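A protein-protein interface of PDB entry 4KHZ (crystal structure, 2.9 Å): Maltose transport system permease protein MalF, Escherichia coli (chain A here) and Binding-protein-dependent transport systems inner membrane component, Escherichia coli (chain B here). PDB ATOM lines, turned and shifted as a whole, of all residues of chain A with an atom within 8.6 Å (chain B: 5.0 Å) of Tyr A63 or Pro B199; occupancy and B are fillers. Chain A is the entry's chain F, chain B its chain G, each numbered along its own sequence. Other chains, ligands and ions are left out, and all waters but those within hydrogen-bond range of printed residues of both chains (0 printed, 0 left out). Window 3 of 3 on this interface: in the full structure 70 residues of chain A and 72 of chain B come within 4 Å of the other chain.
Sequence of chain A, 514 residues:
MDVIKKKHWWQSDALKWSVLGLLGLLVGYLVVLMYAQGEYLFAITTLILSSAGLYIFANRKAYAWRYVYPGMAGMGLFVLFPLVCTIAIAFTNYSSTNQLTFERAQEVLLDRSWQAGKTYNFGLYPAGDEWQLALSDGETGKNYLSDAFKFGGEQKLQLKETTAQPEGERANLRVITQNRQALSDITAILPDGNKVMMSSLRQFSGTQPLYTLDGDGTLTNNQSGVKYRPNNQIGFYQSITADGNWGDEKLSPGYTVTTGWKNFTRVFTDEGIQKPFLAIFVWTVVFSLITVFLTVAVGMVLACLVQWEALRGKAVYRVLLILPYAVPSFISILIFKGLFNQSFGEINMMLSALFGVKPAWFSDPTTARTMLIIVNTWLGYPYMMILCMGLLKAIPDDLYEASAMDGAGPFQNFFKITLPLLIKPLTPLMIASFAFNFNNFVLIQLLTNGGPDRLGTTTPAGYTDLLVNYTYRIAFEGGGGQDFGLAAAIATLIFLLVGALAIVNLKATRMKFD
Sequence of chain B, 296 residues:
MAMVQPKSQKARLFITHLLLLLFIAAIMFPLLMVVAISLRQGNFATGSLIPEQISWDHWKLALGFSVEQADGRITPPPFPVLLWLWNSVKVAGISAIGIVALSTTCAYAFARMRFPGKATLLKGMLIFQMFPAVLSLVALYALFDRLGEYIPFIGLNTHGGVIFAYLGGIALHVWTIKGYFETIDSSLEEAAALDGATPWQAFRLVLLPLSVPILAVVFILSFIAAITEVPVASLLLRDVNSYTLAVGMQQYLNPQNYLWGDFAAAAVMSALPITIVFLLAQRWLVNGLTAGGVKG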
ATOM      1  N   TYR A  55      22.340   2.759   2.694  1.00  0.00           N
ATOM      2  CA  TYR A  55      23.738   2.639   3.115  1.00  0.00           C
ATOM      3  C   TYR A  55      24.691   2.606   1.916  1.00  0.00           C
ATOM      4  O   TYR A  55      25.764   3.207   1.955  1.00  0.00           O
ATOM      5  CB  TYR A  55      23.913   1.374   3.968  1.00  0.00           C
ATOM      6  CG  TYR A  55      25.332   1.052   4.387  1.00  0.00           C
ATOM      7  CD1 TYR A  55      25.838   1.496   5.606  1.00  0.00           C
ATOM      8  CD2 TYR A  55      26.159   0.278   3.575  1.00  0.00           C
ATOM      9  CE1 TYR A  55      27.132   1.193   5.997  1.00  0.00           C
ATOM     10  CE2 TYR A  55      27.454  -0.028   3.957  1.00  0.00           C
ATOM     11  CZ  TYR A  55      27.936   0.431   5.167  1.00  0.00           C
ATOM     12  OH  TYR A  55      29.222   0.127   5.547  1.00  0.00           O
ATOM     13  N   ILE A  56      24.290   1.908   0.858  1.00  0.00           N
ATOM     14  CA  ILE A  56      25.126   1.745  -0.331  1.00  0.00           C
ATOM     15  C   ILE A  56      25.043   2.962  -1.256  1.00  0.00           C
ATOM     16  O   ILE A  56      26.068   3.551  -1.606  1.00  0.00           O
ATOM     17  CB  ILE A  56      24.743   0.460  -1.105  1.00  0.00           C
ATOM     18  CG1 ILE A  56      25.156  -0.782  -0.305  1.00  0.00           C
ATOM     19  CG2 ILE A  56      25.407   0.425  -2.477  1.00  0.00           C
ATOM     20  CD1 ILE A  56      24.401  -2.038  -0.685  1.00  0.00           C
ATOM     21  N   PHE A  57      23.825   3.340  -1.638  1.00  0.00           N
ATOM     22  CA  PHE A  57      23.612   4.361  -2.677  1.00  0.00           C
ATOM     23  C   PHE A  57      23.977   5.786  -2.223  1.00  0.00           C
ATOM     24  O   PHE A  57      24.190   6.665  -3.060  1.00  0.00           O
ATOM     25  CB  PHE A  57      22.157   4.321  -3.182  1.00  0.00           C
ATOM     26  CG  PHE A  57      22.021   4.483  -4.675  1.00  0.00           C
ATOM     27  CD1 PHE A  57      21.821   3.375  -5.492  1.00  0.00           C
ATOM     28  CD2 PHE A  57      22.089   5.740  -5.266  1.00  0.00           C
ATOM     29  CE1 PHE A  57      21.693   3.517  -6.865  1.00  0.00           C
ATOM     30  CE2 PHE A  57      21.963   5.887  -6.639  1.00  0.00           C
ATOM     31  CZ  PHE A  57      21.763   4.776  -7.440  1.00  0.00           C
ATOM     32  N   ALA A  58      24.054   6.014  -0.911  1.00  0.00           N
ATOM     33  CA  ALA A  58      24.366   7.345  -0.376  1.00  0.00           C
ATOM     34  C   ALA A  58      25.823   7.742  -0.624  1.00  0.00           C
ATOM     35  O   ALA A  58      26.092   8.668  -1.392  1.00  0.00           O
ATOM     36  CB  ALA A  58      24.041   7.416   1.111  1.00  0.00           C
ATOM     37  N   ASN A  59      26.751   7.046   0.030  1.00  0.00           N
ATOM     38  CA  ASN A  59      28.184   7.331  -0.116  1.00  0.00           C
ATOM     39  C   ASN A  59      28.768   6.679  -1.369  1.00  0.00           C
ATOM     40  O   ASN A  59      28.162   5.768  -1.943  1.00  0.00           O
ATOM     41  CB  ASN A  59      28.963   6.883   1.131  1.00  0.00           C
ATOM     42  CG  ASN A  59      28.987   5.373   1.305  1.00  0.00           C
ATOM     43  OD1 ASN A  59      28.068   4.671   0.885  1.00  0.00           O
ATOM     44  ND2 ASN A  59      30.040   4.867   1.936  1.00  0.00           N
ATOM     45  N   ARG A  60      29.943   7.150  -1.787  1.00  0.00           N
ATOM     46  CA  ARG A  60      30.617   6.620  -2.977  1.00  0.00           C
ATOM     47  C   ARG A  60      31.900   5.856  -2.626  1.00  0.00           C
ATOM     48  O   ARG A  60      32.860   5.845  -3.401  1.00  0.00           O
ATOM     49  CB  ARG A  60      30.904   7.744  -3.982  1.00  0.00           C
ATOM     50  CG  ARG A  60      29.677   8.576  -4.337  1.00  0.00           C
ATOM     51  CD  ARG A  60      29.544   8.833  -5.833  1.00  0.00           C
ATOM     52  NE  ARG A  60      28.252   9.435  -6.164  1.00  0.00           N
ATOM     53  CZ  ARG A  60      27.813   9.671  -7.401  1.00  0.00           C
ATOM     54  NH1 ARG A  60      28.556   9.359  -8.460  1.00  0.00           N
ATOM     55  NH2 ARG A  60      26.618  10.222  -7.581  1.00  0.00           N
ATOM     56  N   LYS A  61      31.905   5.217  -1.456  1.00  0.00           N
ATOM     57  CA  LYS A  61      32.969   4.289  -1.074  1.00  0.00           C
ATOM     58  C   LYS A  61      32.564   2.868  -1.461  1.00  0.00           C
ATOM     59  O   LYS A  61      33.379   2.104  -1.976  1.00  0.00           O
ATOM     60  CB  LYS A  61      33.253   4.371   0.428  1.00  0.00           C
ATOM     61  CG  LYS A  61      33.787   5.721   0.882  1.00  0.00           C
ATOM     62  CD  LYS A  61      34.154   5.712   2.357  1.00  0.00           C
ATOM     63  CE  LYS A  61      34.748   7.044   2.788  1.00  0.00           C
ATOM     64  NZ  LYS A  61      35.210   7.018   4.202  1.00  0.00           N
ATOM     65  N   ALA A  62      31.301   2.528  -1.205  1.00  0.00           N
ATOM     66  CA  ALA A  62      30.723   1.258  -1.644  1.00  0.00           C
ATOM     67  C   ALA A  62      29.988   1.457  -2.974  1.00  0.00           C
ATOM     68  O   ALA A  62      28.766   1.326  -3.053  1.00  0.00           O
ATOM     69  CB  ALA A  62      29.784   0.710  -0.579  1.00  0.00           C
ATOM     70  N   TYR A  63      30.753   1.777  -4.014  1.00  0.00           N
ATOM     71  CA  TYR A  63      30.203   2.064  -5.339  1.00  0.00           C
ATOM     72  C   TYR A  63      29.845   0.787  -6.098  1.00  0.00           C
ATOM     73  O   TYR A  63      28.846   0.750  -6.815  1.00  0.00           O
ATOM     74  CB  TYR A  63      31.207   2.892  -6.154  1.00  0.00           C
ATOM     75  CG  TYR A  63      30.728   3.290  -7.535  1.00  0.00           C
ATOM     76  CD1 TYR A  63      29.886   4.386  -7.714  1.00  0.00           C
ATOM     77  CD2 TYR A  63      31.129   2.582  -8.664  1.00  0.00           C
ATOM     78  CE1 TYR A  63      29.450   4.757  -8.977  1.00  0.00           C
ATOM     79  CE2 TYR A  63      30.701   2.947  -9.930  1.00  0.00           C
ATOM     80  CZ  TYR A  63      29.861   4.034 -10.083  1.00  0.00           C
ATOM     81  OH  TYR A  63      29.428   4.400 -11.338  1.00  0.00           O
ATOM     82  N   ALA A  64      30.664  -0.252  -5.940  1.00  0.00           N
ATOM     83  CA  ALA A  64      30.462  -1.521  -6.648  1.00  0.00           C
ATOM     84  C   ALA A  64      29.149  -2.207  -6.270  1.00  0.00           C
ATOM     85  O   ALA A  64      28.521  -2.856  -7.109  1.00  0.00           O
ATOM     86  CB  ALA A  64      31.632  -2.460  -6.392  1.00  0.00           C
ATOM     87  N   TRP A  65      28.733  -2.055  -5.014  1.00  0.00           N
ATOM     88  CA  TRP A  65      27.508  -2.688  -4.523  1.00  0.00           C
ATOM     89  C   TRP A  65      26.231  -2.044  -5.075  1.00  0.00           C
ATOM     90  O   TRP A  65      25.158  -2.640  -4.990  1.00  0.00           O
ATOM     91  CB  TRP A  65      27.482  -2.683  -2.991  1.00  0.00           C
ATOM     92  CG  TRP A  65      28.578  -3.506  -2.382  1.00  0.00           C
ATOM     93  CD1 TRP A  65      29.770  -3.052  -1.894  1.00  0.00           C
ATOM     94  CD2 TRP A  65      28.590  -4.927  -2.210  1.00  0.00           C
ATOM     95  NE1 TRP A  65      30.521  -4.102  -1.423  1.00  0.00           N
ATOM     96  CE2 TRP A  65      29.821  -5.266  -1.605  1.00  0.00           C
ATOM     97  CE3 TRP A  65      27.679  -5.949  -2.505  1.00  0.00           C
ATOM     98  CZ2 TRP A  65      30.163  -6.584  -1.290  1.00  0.00           C
ATOM     99  CZ3 TRP A  65      28.021  -7.260  -2.192  1.00  0.00           C
ATOM    100  CH2 TRP A  65      29.252  -7.564  -1.591  1.00  0.00           C
ATOM    101  N   ARG A  66      26.344  -0.841  -5.637  1.00  0.00           N
ATOM    102  CA  ARG A  66      25.200  -0.158  -6.253  1.00  0.00           C
ATOM    103  C   ARG A  66      24.658  -0.934  -7.454  1.00  0.00           C
ATOM    104  O   ARG A  66      23.452  -0.962  -7.695  1.00  0.00           O
ATOM    105  CB  ARG A  66      25.585   1.257  -6.695  1.00  0.00           C
ATOM    106  CG  ARG A  66      25.978   2.182  -5.553  1.00  0.00           C
ATOM    107  CD  ARG A  66      26.326   3.574  -6.053  1.00  0.00           C
ATOM    108  NE  ARG A  66      26.439   4.535  -4.956  1.00  0.00           N
ATOM    109  CZ  ARG A  66      26.587   5.850  -5.109  1.00  0.00           C
ATOM    110  NH1 ARG A  66      26.645   6.393  -6.321  1.00  0.00           N
ATOM    111  NH2 ARG A  66      26.675   6.632  -4.038  1.00  0.00           N
ATOM    112  N   TYR A  67      25.561  -1.563  -8.200  1.00  0.00           N
ATOM    113  CA  TYR A  67      25.197  -2.350  -9.375  1.00  0.00           C
ATOM    114  C   TYR A  67      24.695  -3.746  -9.002  1.00  0.00           C
ATOM    115  O   TYR A  67      23.938  -4.355  -9.756  1.00  0.00           O
ATOM    116  CB  TYR A  67      26.397  -2.473 -10.313  1.00  0.00           C
ATOM    117  CG  TYR A  67      26.810  -1.170 -10.962  1.00  0.00           C
ATOM    118  CD1 TYR A  67      26.427  -0.867 -12.265  1.00  0.00           C
ATOM    119  CD2 TYR A  67      27.586  -0.244 -10.275  1.00  0.00           C
ATOM    120  CE1 TYR A  67      26.805   0.323 -12.865  1.00  0.00           C
ATOM    121  CE2 TYR A  67      27.968   0.948 -10.865  1.00  0.00           C
ATOM    122  CZ  TYR A  67      27.576   1.228 -12.160  1.00  0.00           C
ATOM    123  OH  TYR A  67      27.957   2.412 -12.749  1.00  0.00           O
ATOM    124  N   VAL A  68      25.125  -4.244  -7.843  1.00  0.00           N
ATOM    125  CA  VAL A  68      24.796  -5.596  -7.383  1.00  0.00           C
ATOM    126  C   VAL A  68      23.552  -5.622  -6.486  1.00  0.00           C
ATOM    127  O   VAL A  68      22.792  -6.594  -6.503  1.00  0.00           O
ATOM    128  CB  VAL A  68      25.989  -6.217  -6.620  1.00  0.00           C
ATOM    129  CG1 VAL A  68      25.664  -7.629  -6.146  1.00  0.00           C
ATOM    130  CG2 VAL A  68      27.234  -6.221  -7.498  1.00  0.00           C
ATOM    131  N   TYR A  69      23.353  -4.557  -5.710  1.00  0.00           N
ATOM    132  CA  TYR A  69      22.242  -4.465  -4.754  1.00  0.00           C
ATOM    133  C   TYR A  69      20.865  -4.821  -5.333  1.00  0.00           C
ATOM    134  O   TYR A  69      20.209  -5.731  -4.823  1.00  0.00           O
ATOM    135  CB  TYR A  69      22.201  -3.069  -4.118  1.00  0.00           C
ATOM    136  CG  TYR A  69      21.020  -2.817  -3.200  1.00  0.00           C
ATOM    137  CD1 TYR A  69      21.064  -3.195  -1.860  1.00  0.00           C
ATOM    138  CD2 TYR A  69      19.869  -2.185  -3.667  1.00  0.00           C
ATOM    139  CE1 TYR A  69      19.992  -2.960  -1.013  1.00  0.00           C
ATOM    140  CE2 TYR A  69      18.792  -1.947  -2.827  1.00  0.00           C
ATOM    141  CZ  TYR A  69      18.856  -2.337  -1.503  1.00  0.00           C
ATOM    142  OH  TYR A  69      17.790  -2.100  -0.665  1.00  0.00           O
ATOM    143  N   TYR B 108      27.957  -6.470 -14.653  1.00  0.00           N
ATOM    144  CA  TYR B 108      28.961  -5.439 -14.913  1.00  0.00           C
ATOM    145  C   TYR B 108      29.916  -5.297 -13.730  1.00  0.00           C
ATOM    146  O   TYR B 108      31.118  -5.107 -13.918  1.00  0.00           O
ATOM    147  CB  TYR B 108      28.279  -4.100 -15.213  1.00  0.00           C
ATOM    148  CG  TYR B 108      29.226  -2.950 -15.488  1.00  0.00           C
ATOM    149  CD1 TYR B 108      30.216  -3.052 -16.459  1.00  0.00           C
ATOM    150  CD2 TYR B 108      29.115  -1.749 -14.790  1.00  0.00           C
ATOM    151  CE1 TYR B 108      31.079  -1.999 -16.719  1.00  0.00           C
ATOM    152  CE2 TYR B 108      29.974  -0.692 -15.041  1.00  0.00           C
ATOM    153  CZ  TYR B 108      30.951  -0.822 -16.008  1.00  0.00           C
ATOM    154  OH  TYR B 108      31.804   0.228 -16.260  1.00  0.00           O
ATOM    155  N   MET B 113      34.496  -4.644 -11.832  1.00  0.00           N
ATOM    156  CA  MET B 113      34.810  -4.123 -10.501  1.00  0.00           C
ATOM    157  C   MET B 113      35.310  -5.209  -9.553  1.00  0.00           C
ATOM    158  O   MET B 113      34.876  -6.357  -9.623  1.00  0.00           O
ATOM    159  CB  MET B 113      33.582  -3.431  -9.899  1.00  0.00           C
ATOM    160  CG  MET B 113      33.358  -2.021 -10.422  1.00  0.00           C
ATOM    161  SD  MET B 113      31.623  -1.539 -10.444  1.00  0.00           S
ATOM    162  CE  MET B 113      31.203  -1.921 -12.139  1.00  0.00           C
ATOM    163  N   ALA B 197      35.218   9.210 -18.820  1.00  0.00           N
ATOM    164  CA  ALA B 197      33.914   8.599 -18.598  1.00  0.00           C
ATOM    165  C   ALA B 197      33.899   7.837 -17.276  1.00  0.00           C
ATOM    166  O   ALA B 197      34.787   7.028 -17.005  1.00  0.00           O
ATOM    167  CB  ALA B 197      33.563   7.666 -19.748  1.00  0.00           C
ATOM    168  N   THR B 198      32.884   8.105 -16.458  1.00  0.00           N
ATOM    169  CA  THR B 198      32.688   7.395 -15.197  1.00  0.00           C
ATOM    170  C   THR B 198      32.334   5.933 -15.474  1.00  0.00           C
ATOM    171  O   THR B 198      31.995   5.585 -16.609  1.00  0.00           O
ATOM    172  CB  THR B 198      31.560   8.042 -14.370  1.00  0.00           C
ATOM    173  OG1 THR B 198      30.364   8.116 -15.157  1.00  0.00           O
ATOM    174  CG2 THR B 198      31.959   9.440 -13.924  1.00  0.00           C
ATOM    175  N   PRO B 199      32.420   5.067 -14.445  1.00  0.00           N
ATOM    176  CA  PRO B 199      32.052   3.661 -14.646  1.00  0.00           C
ATOM    177  C   PRO B 199      30.660   3.481 -15.254  1.00  0.00           C
ATOM    178  O   PRO B 199      30.477   2.619 -16.112  1.00  0.00           O
ATOM    179  CB  PRO B 199      32.101   3.081 -13.231  1.00  0.00           C
ATOM    180  CG  PRO B 199      33.102   3.921 -12.519  1.00  0.00           C
ATOM    181  CD  PRO B 199      32.963   5.303 -13.093  1.00  0.00           C
ATOM    182  N   TRP B 200      29.700   4.293 -14.815  1.00  0.00           N
ATOM    183  CA  TRP B 200      28.350   4.263 -15.374  1.00  0.00           C
ATOM    184  C   TRP B 200      28.345   4.680 -16.842  1.00  0.00           C
ATOM    185  O   TRP B 200      27.752   4.003 -17.681  1.00  0.00           O
ATOM    186  CB  TRP B 200      27.405   5.170 -14.583  1.00  0.00           C
ATOM    187  CG  TRP B 200      26.042   5.262 -15.200  1.00  0.00           C
ATOM    188  CD1 TRP B 200      25.553   6.286 -15.961  1.00  0.00           C
ATOM    189  CD2 TRP B 200      25.000   4.278 -15.136  1.00  0.00           C
ATOM    190  NE1 TRP B 200      24.269   6.007 -16.365  1.00  0.00           N
ATOM    191  CE2 TRP B 200      23.905   4.781 -15.873  1.00  0.00           C
ATOM    192  CE3 TRP B 200      24.884   3.024 -14.522  1.00  0.00           C
ATOM    193  CZ2 TRP B 200      22.707   4.072 -16.012  1.00  0.00           C
ATOM    194  CZ3 TRP B 200      23.693   2.320 -14.663  1.00  0.00           C
ATOM    195  CH2 TRP B 200      22.620   2.848 -15.402  1.00  0.00           C
ATOM    196  N   GLN B 201      29.001   5.795 -17.147  1.00  0.00           N
ATOM    197  CA  GLN B 201      29.094   6.282 -18.526  1.00  0.00           C
ATOM    198  C   GLN B 201      29.749   5.264 -19.457  1.00  0.00           C
ATOM    199  O   GLN B 201      29.426   5.215 -20.642  1.00  0.00           O
ATOM    200  CB  GLN B 201      29.861   7.603 -18.580  1.00  0.00           C
ATOM    201  CG  GLN B 201      29.080   8.777 -18.019  1.00  0.00           C
ATOM    202  CD  GLN B 201      29.940  10.003 -17.806  1.00  0.00           C
ATOM    203  OE1 GLN B 201      31.006   9.931 -17.197  1.00  0.00           O
ATOM    204  NE2 GLN B 201      29.474  11.144 -18.299  1.00  0.00           N
ATOM    205  N   ALA B 202      30.670   4.465 -18.921  1.00  0.00           N
ATOM    206  CA  ALA B 202      31.263   3.350 -19.664  1.00  0.00           C
ATOM    207  C   ALA B 202      30.241   2.225 -19.851  1.00  0.00           C
ATOM    208  O   ALA B 202      30.118   1.652 -20.937  1.00  0.00           O
ATOM    209  CB  ALA B 202      32.496   2.827 -18.941  1.00  0.00           C
ATOM    210  N   PHE B 203      29.517   1.916 -18.778  1.00  0.00           N
ATOM    211  CA  PHE B 203      28.457   0.917 -18.818  1.00  0.00           C
ATOM    212  C   PHE B 203      27.428   1.288 -19.878  1.00  0.00           C
ATOM    213  O   PHE B 203      27.120   0.489 -20.761  1.00  0.00           O
ATOM    214  CB  PHE B 203      27.791   0.810 -17.442  1.00  0.00           C
ATOM    215  CG  PHE B 203      26.718  -0.241 -17.354  1.00  0.00           C
ATOM    216  CD1 PHE B 203      25.446   0.086 -16.900  1.00  0.00           C
ATOM    217  CD2 PHE B 203      26.979  -1.557 -17.712  1.00  0.00           C
ATOM    218  CE1 PHE B 203      24.456  -0.878 -16.808  1.00  0.00           C
ATOM    219  CE2 PHE B 203      25.990  -2.526 -17.626  1.00  0.00           C
ATOM    220  CZ  PHE B 203      24.726  -2.186 -17.172  1.00  0.00           C
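Hydrophobic or aromatic side chains of chain B within 4 Å of the printed part of chain A: Tyr B108, Met B113, Pro B199 and Trp B200. Among the printed residues, 6 pairs touch across the chains. Among the printed residues, no Asp or Glu carboxylate lies within 4 Å of a Lys or Arg side-chain nitrogen of the other chain.
OH of Tyr A63 sits at hydrogen-bond distance from OH of Tyr A67. The side-chain hydroxyl (OH) of Tyr B108 lies within hydrogen-bond range of the backbone carbonyl oxygen (O) of Pro B199, at 2.7 Å.
Tyr A55 touches none of the printed residues of chain B. Ala A62 touches none of the printed residues of chain B. Of the printed residues of chain B, Tyr A63 touches Pro B199 (3.5 Å) and Trp B200 (3.5 Å). Printed residues of chain B within 4 Å of Ala A64: Met B113 (3.97 Å). Printed residues of chain B within 4 Å of Tyr A67: Tyr B108 (3.7 Å), Pro B199 (3.8 Å) and Trp B200 (3.2 Å). Printed residues of chain A within 4 Å of Met B113: Ala A64 (3.97 Å). No residue of chain A comes within 4 Å of Thr B198. Pro B199 touches just these residues of chain A: Tyr A63 (3.5 Å) and Tyr A67 (3.8 Å). Of the printed residues of chain A, Trp B200 touches Tyr A63 (3.5 Å) and Tyr A67 (3.2 Å). The nearest residue of chain A that does not touch Pro B199 is Arg A60 (7.6 Å). The nearest printed residue of chain A that does not touch Trp B200 is Arg A60 (7.5 Å).
Tyr A63 touches Pro B199 (OH to CB, 3.5 Å). CA of Ala A64 touches SD of Met B113, 3.97 Å away. Tyr A67 touches Tyr B108. OH of Tyr A67 touches C of Pro B199, 3.8 Å away.
N of Trp B200 lies close to OH of Tyr A67. The backbone NH (N) of Trp B200 is in hydrogen-bond range of the side-chain hydroxyl (OH) of Tyr A63.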
